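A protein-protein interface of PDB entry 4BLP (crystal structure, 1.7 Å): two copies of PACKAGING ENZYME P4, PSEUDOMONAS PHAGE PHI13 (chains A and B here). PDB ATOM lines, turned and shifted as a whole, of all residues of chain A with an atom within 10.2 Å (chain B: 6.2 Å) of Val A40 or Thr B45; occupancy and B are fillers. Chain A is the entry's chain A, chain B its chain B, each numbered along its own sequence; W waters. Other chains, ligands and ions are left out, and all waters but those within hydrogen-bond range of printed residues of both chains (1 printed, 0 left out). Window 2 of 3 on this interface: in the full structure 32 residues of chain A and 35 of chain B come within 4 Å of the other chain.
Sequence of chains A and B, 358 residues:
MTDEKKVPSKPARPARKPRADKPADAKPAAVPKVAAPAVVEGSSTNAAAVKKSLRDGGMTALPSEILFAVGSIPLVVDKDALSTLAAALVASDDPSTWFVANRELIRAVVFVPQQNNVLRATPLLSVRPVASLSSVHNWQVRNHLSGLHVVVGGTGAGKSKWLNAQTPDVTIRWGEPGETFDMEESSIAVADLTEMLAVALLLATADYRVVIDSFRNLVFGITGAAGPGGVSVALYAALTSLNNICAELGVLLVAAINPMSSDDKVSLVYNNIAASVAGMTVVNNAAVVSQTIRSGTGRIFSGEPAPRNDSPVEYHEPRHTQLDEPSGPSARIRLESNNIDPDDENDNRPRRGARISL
The side-chain amide nitrogen (NE2) of Gln A114 sits at hydrogen-bond distance from the backbone carbonyl oxygen (O) of Arg B120, at 3.2 Å.
The side-chain hydroxyl of Ser B44 is in hydrogen-bond range of the side-chain carboxylate of Glu A41 (2.6 Å).
NE of Arg B120 lies within hydrogen-bond range of O of Val A39.
The backbone NH of Thr B45 lies within hydrogen-bond range of the side-chain hydroxyl of Ser B43, 3.1 Å away.
NH2 of Arg B120 sits at hydrogen-bond distance from OE1 of Gln B115 (2.9 Å).
The side-chain amide nitrogen of Gln A114 lies within hydrogen-bond range of the backbone carbonyl oxygen of Val A112 (3.1 Å).
N of Gly A42 sits at hydrogen-bond distance from O of Gln A114 (2.9 Å).
Among the printed residues, merely in contact across the chains: Glu A41 with Arg B120, Val A112 with Arg B120, Val A40 with Thr B45, Val A39 with Val B50, Val A40 with Ala B47, Val A40 with Ser B44, Val A40 with Val B50 and Glu A41 with Thr B45.
Ala A38 touches none of the printed residues of chain B.
Printed residues of chain B within 4 Å of Val A39: Val B50 and Arg B120.
Val A40 touches just these residues of chain B: Ser B44, Thr B45, Ala B47 and Val B50.
Of the printed residues of chain B, Glu A41 touches Ser B44 (2.6 Å), Thr B45 (3.9 Å) and Arg B120 (3.5 Å).
Of the printed residues of chain B, Val A112 touches Arg B120.
Of the printed residues of chain B, Gln A114 touches Arg B120 (3.2 Å).
Of the printed residues of chain A, Ser B44 touches Val A40 (3.7 Å) and Glu A41 (2.6 Å).
Of chain A, only Val A40 (3.6 Å) and Glu A41 (3.9 Å) come within 4 Å of Thr B45.
No residue of chain A comes within 4 Å of Asn B46.
Printed residues of chain A within 4 Å of Val B50: Val A39 and Val A40.
Lys B51 touches none of the printed residues of chain A.
The nearest residue of chain B that does not touch Val A40 is Arg B120 (4.3 Å).
Of the 24 printed residues of chain A, 5 touch a printed residue of chain B.
Hydrophobic or aromatic side chains of chain A that line the printed part of chain B: Val A39, Val A40 and Val A112.
Among the printed residues, no Asp or Glu carboxylate lies within 4 Å of a Lys or Arg side-chain nitrogen of the other chain.
5 positions are printed for both chains.
Of the 11 pairs that touch across the chains among the printed residues, none has its exchanged pair printed and touching as well.
Water W1 lies within hydrogen-bond range of O of Glu A41 (2.6 Å) and O of Thr B45 (3.4 Å).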
ATOM      1  N   ALA A  36      16.450  17.791 -24.179  1.00  0.00           N
ATOM      2  CA  ALA A  36      15.680  18.731 -23.372  1.00  0.00           C
ATOM      3  C   ALA A  36      16.517  18.991 -22.138  1.00  0.00           C
ATOM      4  O   ALA A  36      16.832  18.032 -21.436  1.00  0.00           O
ATOM      5  CB  ALA A  36      14.328  18.116 -23.017  1.00  0.00           C
ATOM      6  N   PRO A  37      16.994  20.229 -21.846  1.00  0.00           N
ATOM      7  CA  PRO A  37      17.824  20.407 -20.641  1.00  0.00           C
ATOM      8  C   PRO A  37      17.068  20.034 -19.371  1.00  0.00           C
ATOM      9  O   PRO A  37      15.871  20.264 -19.304  1.00  0.00           O
ATOM     10  CB  PRO A  37      18.190  21.899 -20.662  1.00  0.00           C
ATOM     11  CG  PRO A  37      17.923  22.352 -22.019  1.00  0.00           C
ATOM     12  CD  PRO A  37      16.765  21.514 -22.532  1.00  0.00           C
ATOM     13  N   ALA A  38      17.761  19.454 -18.376  1.00  0.00           N
ATOM     14  CA  ALA A  38      17.158  19.019 -17.114  1.00  0.00           C
ATOM     15  C   ALA A  38      16.646  20.225 -16.340  1.00  0.00           C
ATOM     16  O   ALA A  38      17.291  21.267 -16.371  1.00  0.00           O
ATOM     17  CB  ALA A  38      18.199  18.285 -16.281  1.00  0.00           C
ATOM     18  N   VAL A  39      15.502  20.101 -15.673  1.00  0.00           N
ATOM     19  CA  VAL A  39      15.024  21.205 -14.818  1.00  0.00           C
ATOM     20  C   VAL A  39      15.074  20.744 -13.368  1.00  0.00           C
ATOM     21  O   VAL A  39      15.074  21.587 -12.478  1.00  0.00           O
ATOM     22  CB  VAL A  39      13.664  21.848 -15.194  1.00  0.00           C
ATOM     23  CG1 VAL A  39      13.797  22.689 -16.466  1.00  0.00           C
ATOM     24  CG2 VAL A  39      12.600  20.794 -15.353  1.00  0.00           C
ATOM     25  N   VAL A  40      15.241  19.432 -13.119  1.00  0.00           N
ATOM     26  CA  VAL A  40      15.483  18.923 -11.774  1.00  0.00           C
ATOM     27  C   VAL A  40      16.835  19.499 -11.288  1.00  0.00           C
ATOM     28  O   VAL A  40      17.824  19.479 -12.058  1.00  0.00           O
ATOM     29  CB  VAL A  40      15.508  17.379 -11.751  1.00  0.00           C
ATOM     30  CG1 VAL A  40      15.926  16.849 -10.382  1.00  0.00           C
ATOM     31  CG2 VAL A  40      14.159  16.798 -12.185  1.00  0.00           C
ATOM     32  N   GLU A  41      16.883  20.019 -10.060  1.00  0.00           N
ATOM     33  CA  GLU A  41      18.141  20.570  -9.512  1.00  0.00           C
ATOM     34  C   GLU A  41      19.138  19.436  -9.285  1.00  0.00           C
ATOM     35  O   GLU A  41      18.774  18.402  -8.693  1.00  0.00           O
ATOM     36  CB  GLU A  41      17.907  21.323  -8.191  1.00  0.00           C
ATOM     37  CG  GLU A  41      17.087  22.606  -8.379  1.00  0.00           C
ATOM     38  CD  GLU A  41      16.735  23.285  -7.064  1.00  0.00           C
ATOM     39  OE1 GLU A  41      16.819  22.633  -5.996  1.00  0.00           O
ATOM     40  OE2 GLU A  41      16.277  24.441  -7.111  1.00  0.00           O
ATOM     41  N   GLY A  42      20.362  19.639  -9.762  1.00  0.00           N
ATOM     42  CA  GLY A  42      21.419  18.629  -9.633  1.00  0.00           C
ATOM     43  C   GLY A  42      22.228  18.796  -8.365  1.00  0.00           C
ATOM     44  O   GLY A  42      22.570  19.915  -7.988  1.00  0.00           O
ATOM     45  N   SER A  43      22.552  17.685  -7.701  1.00  0.00           N
ATOM     46  CA  SER A  43      23.321  17.755  -6.454  1.00  0.00           C
ATOM     47  C   SER A  43      24.763  18.215  -6.698  1.00  0.00           C
ATOM     48  O   SER A  43      25.396  17.786  -7.651  1.00  0.00           O
ATOM     49  CB  SER A  43      23.325  16.400  -5.763  1.00  0.00           C
ATOM     50  OG  SER A  43      24.254  16.410  -4.688  1.00  0.00           O
ATOM     51  N   SER A  44      25.281  19.089  -5.830  1.00  0.00           N
ATOM     52  CA  SER A  44      26.680  19.514  -5.947  1.00  0.00           C
ATOM     53  C   SER A  44      27.594  18.694  -5.001  1.00  0.00           C
ATOM     54  O   SER A  44      28.805  18.892  -5.005  1.00  0.00           O
ATOM     55  CB  SER A  44      26.809  21.002  -5.653  1.00  0.00           C
ATOM     56  OG  SER A  44      26.266  21.274  -4.366  1.00  0.00           O
ATOM     57  N   THR A  45      27.021  17.740  -4.227  1.00  0.00           N
ATOM     58  CA  THR A  45      27.799  16.966  -3.262  1.00  0.00           C
ATOM     59  C   THR A  45      27.899  15.497  -3.656  1.00  0.00           C
ATOM     60  O   THR A  45      28.574  14.739  -2.975  1.00  0.00           O
ATOM     61  CB  THR A  45      27.173  17.097  -1.867  1.00  0.00           C
ATOM     62  OG1 THR A  45      25.849  16.564  -1.939  1.00  0.00           O
ATOM     63  CG2 THR A  45      27.124  18.552  -1.367  1.00  0.00           C
ATOM     64  N   ALA A  49      26.294  12.909  -9.877  1.00  0.00           N
ATOM     65  CA  ALA A  49      25.504  14.033 -10.400  1.00  0.00           C
ATOM     66  C   ALA A  49      26.410  15.092 -11.007  1.00  0.00           C
ATOM     67  O   ALA A  49      26.129  15.597 -12.095  1.00  0.00           O
ATOM     68  CB  ALA A  49      24.675  14.654  -9.283  1.00  0.00           C
ATOM     69  N   LYS A  52      27.898  14.643 -14.639  1.00  0.00           N
ATOM     70  CA  LYS A  52      27.002  14.781 -15.792  1.00  0.00           C
ATOM     71  C   LYS A  52      27.218  16.098 -16.534  1.00  0.00           C
ATOM     72  O   LYS A  52      27.845  17.027 -15.996  1.00  0.00           O
ATOM     73  CB  LYS A  52      25.538  14.645 -15.343  1.00  0.00           C
ATOM     74  CG  LYS A  52      25.247  13.217 -14.853  1.00  0.00           C
ATOM     75  CD  LYS A  52      23.783  13.032 -14.512  1.00  0.00           C
ATOM     76  CE  LYS A  52      23.480  11.591 -14.163  1.00  0.00           C
ATOM     77  NZ  LYS A  52      22.060  11.415 -13.761  1.00  0.00           N
ATOM     78  N   SER A  53      26.731  16.162 -17.799  1.00  0.00           N
ATOM     79  CA  SER A  53      26.847  17.374 -18.601  1.00  0.00           C
ATOM     80  C   SER A  53      26.052  18.522 -17.974  1.00  0.00           C
ATOM     81  O   SER A  53      25.180  18.277 -17.131  1.00  0.00           O
ATOM     82  CB  SER A  53      26.322  17.121 -20.012  1.00  0.00           C
ATOM     83  OG  SER A  53      24.932  16.858 -19.970  1.00  0.00           O
ATOM     84  N   LEU A  54      26.309  19.760 -18.417  1.00  0.00           N
ATOM     85  CA  LEU A  54      25.542  20.911 -17.906  1.00  0.00           C
ATOM     86  C   LEU A  54      24.037  20.774 -18.230  1.00  0.00           C
ATOM     87  O   LEU A  54      23.191  21.097 -17.390  1.00  0.00           O
ATOM     88  CB  LEU A  54      26.090  22.206 -18.490  1.00  0.00           C
ATOM     89  CG  LEU A  54      27.476  22.586 -17.907  1.00  0.00           C
ATOM     90  CD1 LEU A  54      28.213  23.549 -18.821  1.00  0.00           C
ATOM     91  CD2 LEU A  54      27.340  23.229 -16.501  1.00  0.00           C
ATOM     92  N   ARG A  55      23.690  20.280 -19.449  1.00  0.00           N
ATOM     93  CA  ARG A  55      22.279  20.066 -19.797  1.00  0.00           C
ATOM     94  C   ARG A  55      21.631  19.015 -18.909  1.00  0.00           C
ATOM     95  O   ARG A  55      20.414  18.986 -18.834  1.00  0.00           O
ATOM     96  CB  ARG A  55      22.139  19.638 -21.285  1.00  0.00           C
ATOM     97  CG  ARG A  55      22.809  18.295 -21.566  1.00  0.00           C
ATOM     98  CD  ARG A  55      22.322  17.664 -22.865  1.00  0.00           C
ATOM     99  NE  ARG A  55      22.927  18.379 -23.977  1.00  0.00           N
ATOM    100  CZ  ARG A  55      23.218  17.849 -25.156  1.00  0.00           C
ATOM    101  NH1 ARG A  55      22.956  16.568 -25.401  1.00  0.00           N
ATOM    102  NH2 ARG A  55      23.791  18.586 -26.095  1.00  0.00           N
ATOM    103  N   ASP A  56      22.415  18.103 -18.309  1.00  0.00           N
ATOM    104  CA  ASP A  56      21.894  17.007 -17.480  1.00  0.00           C
ATOM    105  C   ASP A  56      22.040  17.266 -15.989  1.00  0.00           C
ATOM    106  O   ASP A  56      21.950  16.331 -15.180  1.00  0.00           O
ATOM    107  CB  ASP A  56      22.571  15.678 -17.839  1.00  0.00           C
ATOM    108  CG  ASP A  56      22.186  15.101 -19.184  1.00  0.00           C
ATOM    109  OD1 ASP A  56      21.160  15.549 -19.757  1.00  0.00           O
ATOM    110  OD2 ASP A  56      22.904  14.186 -19.665  1.00  0.00           O
ATOM    111  N   GLY A  57      22.219  18.527 -15.617  1.00  0.00           N
ATOM    112  CA  GLY A  57      22.252  18.874 -14.205  1.00  0.00           C
ATOM    113  C   GLY A  57      23.581  18.748 -13.498  1.00  0.00           C
ATOM    114  O   GLY A  57      23.620  18.944 -12.285  1.00  0.00           O
ATOM    115  N   GLY A  58      24.665  18.463 -14.232  1.00  0.00           N
ATOM    116  CA  GLY A  58      26.015  18.364 -13.674  1.00  0.00           C
ATOM    117  C   GLY A  58      26.908  19.542 -13.992  1.00  0.00           C
ATOM    118  O   GLY A  58      26.425  20.616 -14.386  1.00  0.00           O
ATOM    119  N   PHE A 111      19.939  27.864 -21.906  1.00  0.00           N
ATOM    120  CA  PHE A 111      19.216  27.438 -20.710  1.00  0.00           C
ATOM    121  C   PHE A 111      20.000  27.747 -19.454  1.00  0.00           C
ATOM    122  O   PHE A 111      21.228  27.935 -19.494  1.00  0.00           O
ATOM    123  CB  PHE A 111      18.914  25.928 -20.783  1.00  0.00           C
ATOM    124  CG  PHE A 111      20.151  25.044 -20.888  1.00  0.00           C
ATOM    125  CD1 PHE A 111      20.694  24.726 -22.134  1.00  0.00           C
ATOM    126  CD2 PHE A 111      20.762  24.528 -19.736  1.00  0.00           C
ATOM    127  CE1 PHE A 111      21.860  23.931 -22.230  1.00  0.00           C
ATOM    128  CE2 PHE A 111      21.906  23.725 -19.825  1.00  0.00           C
ATOM    129  CZ  PHE A 111      22.442  23.416 -21.080  1.00  0.00           C
ATOM    130  N   VAL A 112      19.290  27.759 -18.341  1.00  0.00           N
ATOM    131  CA  VAL A 112      19.969  27.867 -17.029  1.00  0.00           C
ATOM    132  C   VAL A 112      20.372  26.438 -16.614  1.00  0.00           C
ATOM    133  O   VAL A 112      19.468  25.574 -16.475  1.00  0.00           O
ATOM    134  CB  VAL A 112      19.043  28.505 -15.959  1.00  0.00           C
ATOM    135  CG1 VAL A 112      19.742  28.488 -14.587  1.00  0.00           C
ATOM    136  CG2 VAL A 112      18.651  29.925 -16.340  1.00  0.00           C
ATOM    137  N   PRO A 113      21.677  26.150 -16.443  1.00  0.00           N
ATOM    138  CA  PRO A 113      22.091  24.804 -16.004  1.00  0.00           C
ATOM    139  C   PRO A 113      21.634  24.646 -14.568  1.00  0.00           C
ATOM    140  O   PRO A 113      21.761  25.595 -13.766  1.00  0.00           O
ATOM    141  CB  PRO A 113      23.614  24.811 -16.183  1.00  0.00           C
ATOM    142  CG  PRO A 113      24.000  26.271 -15.964  1.00  0.00           C
ATOM    143  CD  PRO A 113      22.828  27.071 -16.551  1.00  0.00           C
ATOM    144  N   GLN A 114      21.074  23.470 -14.238  1.00  0.00           N
ATOM    145  CA  GLN A 114      20.443  23.321 -12.936  1.00  0.00           C
ATOM    146  C   GLN A 114      21.269  22.612 -11.876  1.00  0.00           C
ATOM    147  O   GLN A 114      20.771  22.376 -10.766  1.00  0.00           O
ATOM    148  CB  GLN A 114      19.062  22.654 -13.089  1.00  0.00           C
ATOM    149  CG  GLN A 114      18.061  23.552 -13.877  1.00  0.00           C
ATOM    150  CD  GLN A 114      17.813  24.912 -13.234  1.00  0.00           C
ATOM    151  OE1 GLN A 114      17.920  25.099 -12.015  1.00  0.00           O
ATOM    152  NE2 GLN A 114      17.522  25.923 -14.031  1.00  0.00           N
ATOM    153  N   GLN A 115      22.562  22.387 -12.158  1.00  0.00           N
ATOM    154  CA  GLN A 115      23.476  21.952 -11.107  1.00  0.00           C
ATOM    155  C   GLN A 115      23.445  22.972  -9.961  1.00  0.00           C
ATOM    156  O   GLN A 115      23.564  24.185 -10.192  1.00  0.00           O
ATOM    157  CB  GLN A 115      24.887  21.854 -11.693  1.00  0.00           C
ATOM    158  CG  GLN A 115      26.043  21.864 -10.696  1.00  0.00           C
ATOM    159  CD  GLN A 115      26.255  20.614  -9.858  1.00  0.00           C
ATOM    160  OE1 GLN A 115      27.083  20.641  -8.959  1.00  0.00           O
ATOM    161  NE2 GLN A 115      25.543  19.498 -10.104  1.00  0.00           N
ATOM    162  N   ASN A 116      23.328  22.491  -8.733  1.00  0.00           N
ATOM    163  CA  ASN A 116      23.399  23.412  -7.580  1.00  0.00           C
ATOM    164  C   ASN A 116      24.740  24.171  -7.550  1.00  0.00           C
ATOM    165  O   ASN A 116      25.788  23.560  -7.793  1.00  0.00           O
ATOM    166  CB  ASN A 116      23.250  22.621  -6.286  1.00  0.00           C
ATOM    167  CG  ASN A 116      23.206  23.511  -5.060  1.00  0.00           C
ATOM    168  OD1 ASN A 116      22.392  24.427  -4.977  1.00  0.00           O
ATOM    169  ND2 ASN A 116      24.114  23.306  -4.139  1.00  0.00           N
ATOM    170  N   GLY B  42       6.379  21.541  -3.510  1.00  0.00           N
ATOM    171  CA  GLY B  42       6.892  20.500  -4.401  1.00  0.00           C
ATOM    172  C   GLY B  42       8.406  20.423  -4.400  1.00  0.00           C
ATOM    173  O   GLY B  42       9.080  21.447  -4.452  1.00  0.00           O
ATOM    174  N   SER B  43       8.953  19.197  -4.362  1.00  0.00           N
ATOM    175  CA  SER B  43      10.400  19.027  -4.376  1.00  0.00           C
ATOM    176  C   SER B  43      11.003  19.465  -5.730  1.00  0.00           C
ATOM    177  O   SER B  43      10.432  19.167  -6.786  1.00  0.00           O
ATOM    178  CB  SER B  43      10.745  17.559  -4.099  1.00  0.00           C
ATOM    179  OG  SER B  43      12.123  17.339  -4.328  1.00  0.00           O
ATOM    180  N   SER B  44      12.139  20.179  -5.691  1.00  0.00           N
ATOM    181  CA  SER B  44      12.847  20.559  -6.928  1.00  0.00           C
ATOM    182  C   SER B  44      13.961  19.560  -7.252  1.00  0.00           C
ATOM    183  O   SER B  44      14.647  19.719  -8.271  1.00  0.00           O
ATOM    184  CB  SER B  44      13.411  21.979  -6.826  1.00  0.00           C
ATOM    185  OG  SER B  44      14.260  22.107  -5.696  1.00  0.00           O
ATOM    186  N   THR B  45      14.133  18.507  -6.427  1.00  0.00           N
ATOM    187  CA  THR B  45      15.222  17.537  -6.636  1.00  0.00           C
ATOM    188  C   THR B  45      14.702  16.141  -6.974  1.00  0.00           C
ATOM    189  O   THR B  45      15.500  15.239  -7.197  1.00  0.00           O
ATOM    190  CB  THR B  45      16.123  17.476  -5.390  1.00  0.00           C
ATOM    191  OG1 THR B  45      15.292  17.087  -4.294  1.00  0.00           O
ATOM    192  CG2 THR B  45      16.787  18.820  -5.076  1.00  0.00           C
ATOM    193  N   ASN B  46      13.373  15.961  -6.981  1.00  0.00           N
ATOM    194  CA  ASN B  46      12.721  14.689  -7.282  1.00  0.00           C
ATOM    195  C   ASN B  46      12.104  14.797  -8.698  1.00  0.00           C
ATOM    196  O   ASN B  46      11.233  15.640  -8.927  1.00  0.00           O
ATOM    197  CB  ASN B  46      11.675  14.400  -6.189  1.00  0.00           C
ATOM    198  CG  ASN B  46      10.894  13.139  -6.431  1.00  0.00           C
ATOM    199  OD1 ASN B  46       9.945  13.118  -7.209  1.00  0.00           O
ATOM    200  ND2 ASN B  46      11.281  12.059  -5.780  1.00  0.00           N
ATOM    201  N   ALA B  47      12.571  13.967  -9.644  1.00  0.00           N
ATOM    202  CA  ALA B  47      12.082  14.007 -11.023  1.00  0.00           C
ATOM    203  C   ALA B  47      10.555  13.832 -11.126  1.00  0.00           C
ATOM    204  O   ALA B  47       9.938  14.513 -11.945  1.00  0.00           O
ATOM    205  CB  ALA B  47      12.772  12.945 -11.869  1.00  0.00           C
ATOM    206  N   ALA B  48       9.947  12.912 -10.341  1.00  0.00           N
ATOM    207  CA  ALA B  48       8.500  12.688 -10.424  1.00  0.00           C
ATOM    208  C   ALA B  48       7.697  13.956 -10.017  1.00  0.00           C
ATOM    209  O   ALA B  48       6.696  14.302 -10.663  1.00  0.00           O
ATOM    210  CB  ALA B  48       8.103  11.494  -9.560  1.00  0.00           C
ATOM    211  N   VAL B  50       8.881  17.136 -10.125  1.00  0.00           N
ATOM    212  CA  VAL B  50       9.173  18.245 -11.069  1.00  0.00           C
ATOM    213  C   VAL B  50       8.388  18.095 -12.395  1.00  0.00           C
ATOM    214  O   VAL B  50       7.975  19.084 -12.991  1.00  0.00           O
ATOM    215  CB  VAL B  50      10.720  18.298 -11.309  1.00  0.00           C
ATOM    216  CG1 VAL B  50      11.098  19.198 -12.488  1.00  0.00           C
ATOM    217  CG2 VAL B  50      11.471  18.735 -10.037  1.00  0.00           C
ATOM    218  N   LYS B  51       8.148  16.859 -12.829  1.00  0.00           N
ATOM    219  CA  LYS B  51       7.453  16.601 -14.101  1.00  0.00           C
ATOM    220  C   LYS B  51       5.970  17.047 -14.071  1.00  0.00           C
ATOM    221  O   LYS B  51       5.359  17.211 -15.134  1.00  0.00           O
ATOM    222  CB  LYS B  51       7.589  15.102 -14.492  1.00  0.00           C
ATOM    223  CG  LYS B  51       6.606  14.123 -13.894  1.00  0.00           C
ATOM    224  CD  LYS B  51       6.912  12.692 -14.348  1.00  0.00           C
ATOM    225  CE  LYS B  51       6.103  11.788 -13.483  1.00  0.00           C
ATOM    226  NZ  LYS B  51       6.587  10.394 -13.586  1.00  0.00           N
ATOM    227  N   GLN B 115       5.905  24.529  -6.463  1.00  0.00           N
ATOM    228  CA  GLN B 115       7.207  23.911  -6.751  1.00  0.00           C
ATOM    229  C   GLN B 115       8.313  24.752  -6.097  1.00  0.00           C
ATOM    230  O   GLN B 115       8.337  25.976  -6.249  1.00  0.00           O
ATOM    231  CB  GLN B 115       7.428  23.870  -8.282  1.00  0.00           C
ATOM    232  CG  GLN B 115       8.878  23.654  -8.749  1.00  0.00           C
ATOM    233  CD  GLN B 115       9.493  22.287  -8.544  1.00  0.00           C
ATOM    234  OE1 GLN B 115      10.685  22.116  -8.791  1.00  0.00           O
ATOM    235  NE2 GLN B 115       8.743  21.270  -8.112  1.00  0.00           N
ATOM    236  N   ARG B 120      13.470  29.093 -11.348  1.00  0.00           N
ATOM    237  CA  ARG B 120      14.888  28.785 -11.632  1.00  0.00           C
ATOM    238  C   ARG B 120      15.233  28.599 -13.129  1.00  0.00           C
ATOM    239  O   ARG B 120      16.386  28.828 -13.496  1.00  0.00           O
ATOM    240  CB  ARG B 120      15.340  27.540 -10.856  1.00  0.00           C
ATOM    241  CG  ARG B 120      14.665  26.241 -11.293  1.00  0.00           C
ATOM    242  CD  ARG B 120      15.171  25.119 -10.392  1.00  0.00           C
ATOM    243  NE  ARG B 120      14.580  23.824 -10.738  1.00  0.00           N
ATOM    244  CZ  ARG B 120      13.430  23.381 -10.231  1.00  0.00           C
ATOM    245  NH1 ARG B 120      12.722  24.146  -9.403  1.00  0.00           N
ATOM    246  NH2 ARG B 120      12.990  22.158 -10.530  1.00  0.00           N
HETATM  247  O   HOH W   1      18.769  16.025  -7.596  1.00  0.00           O
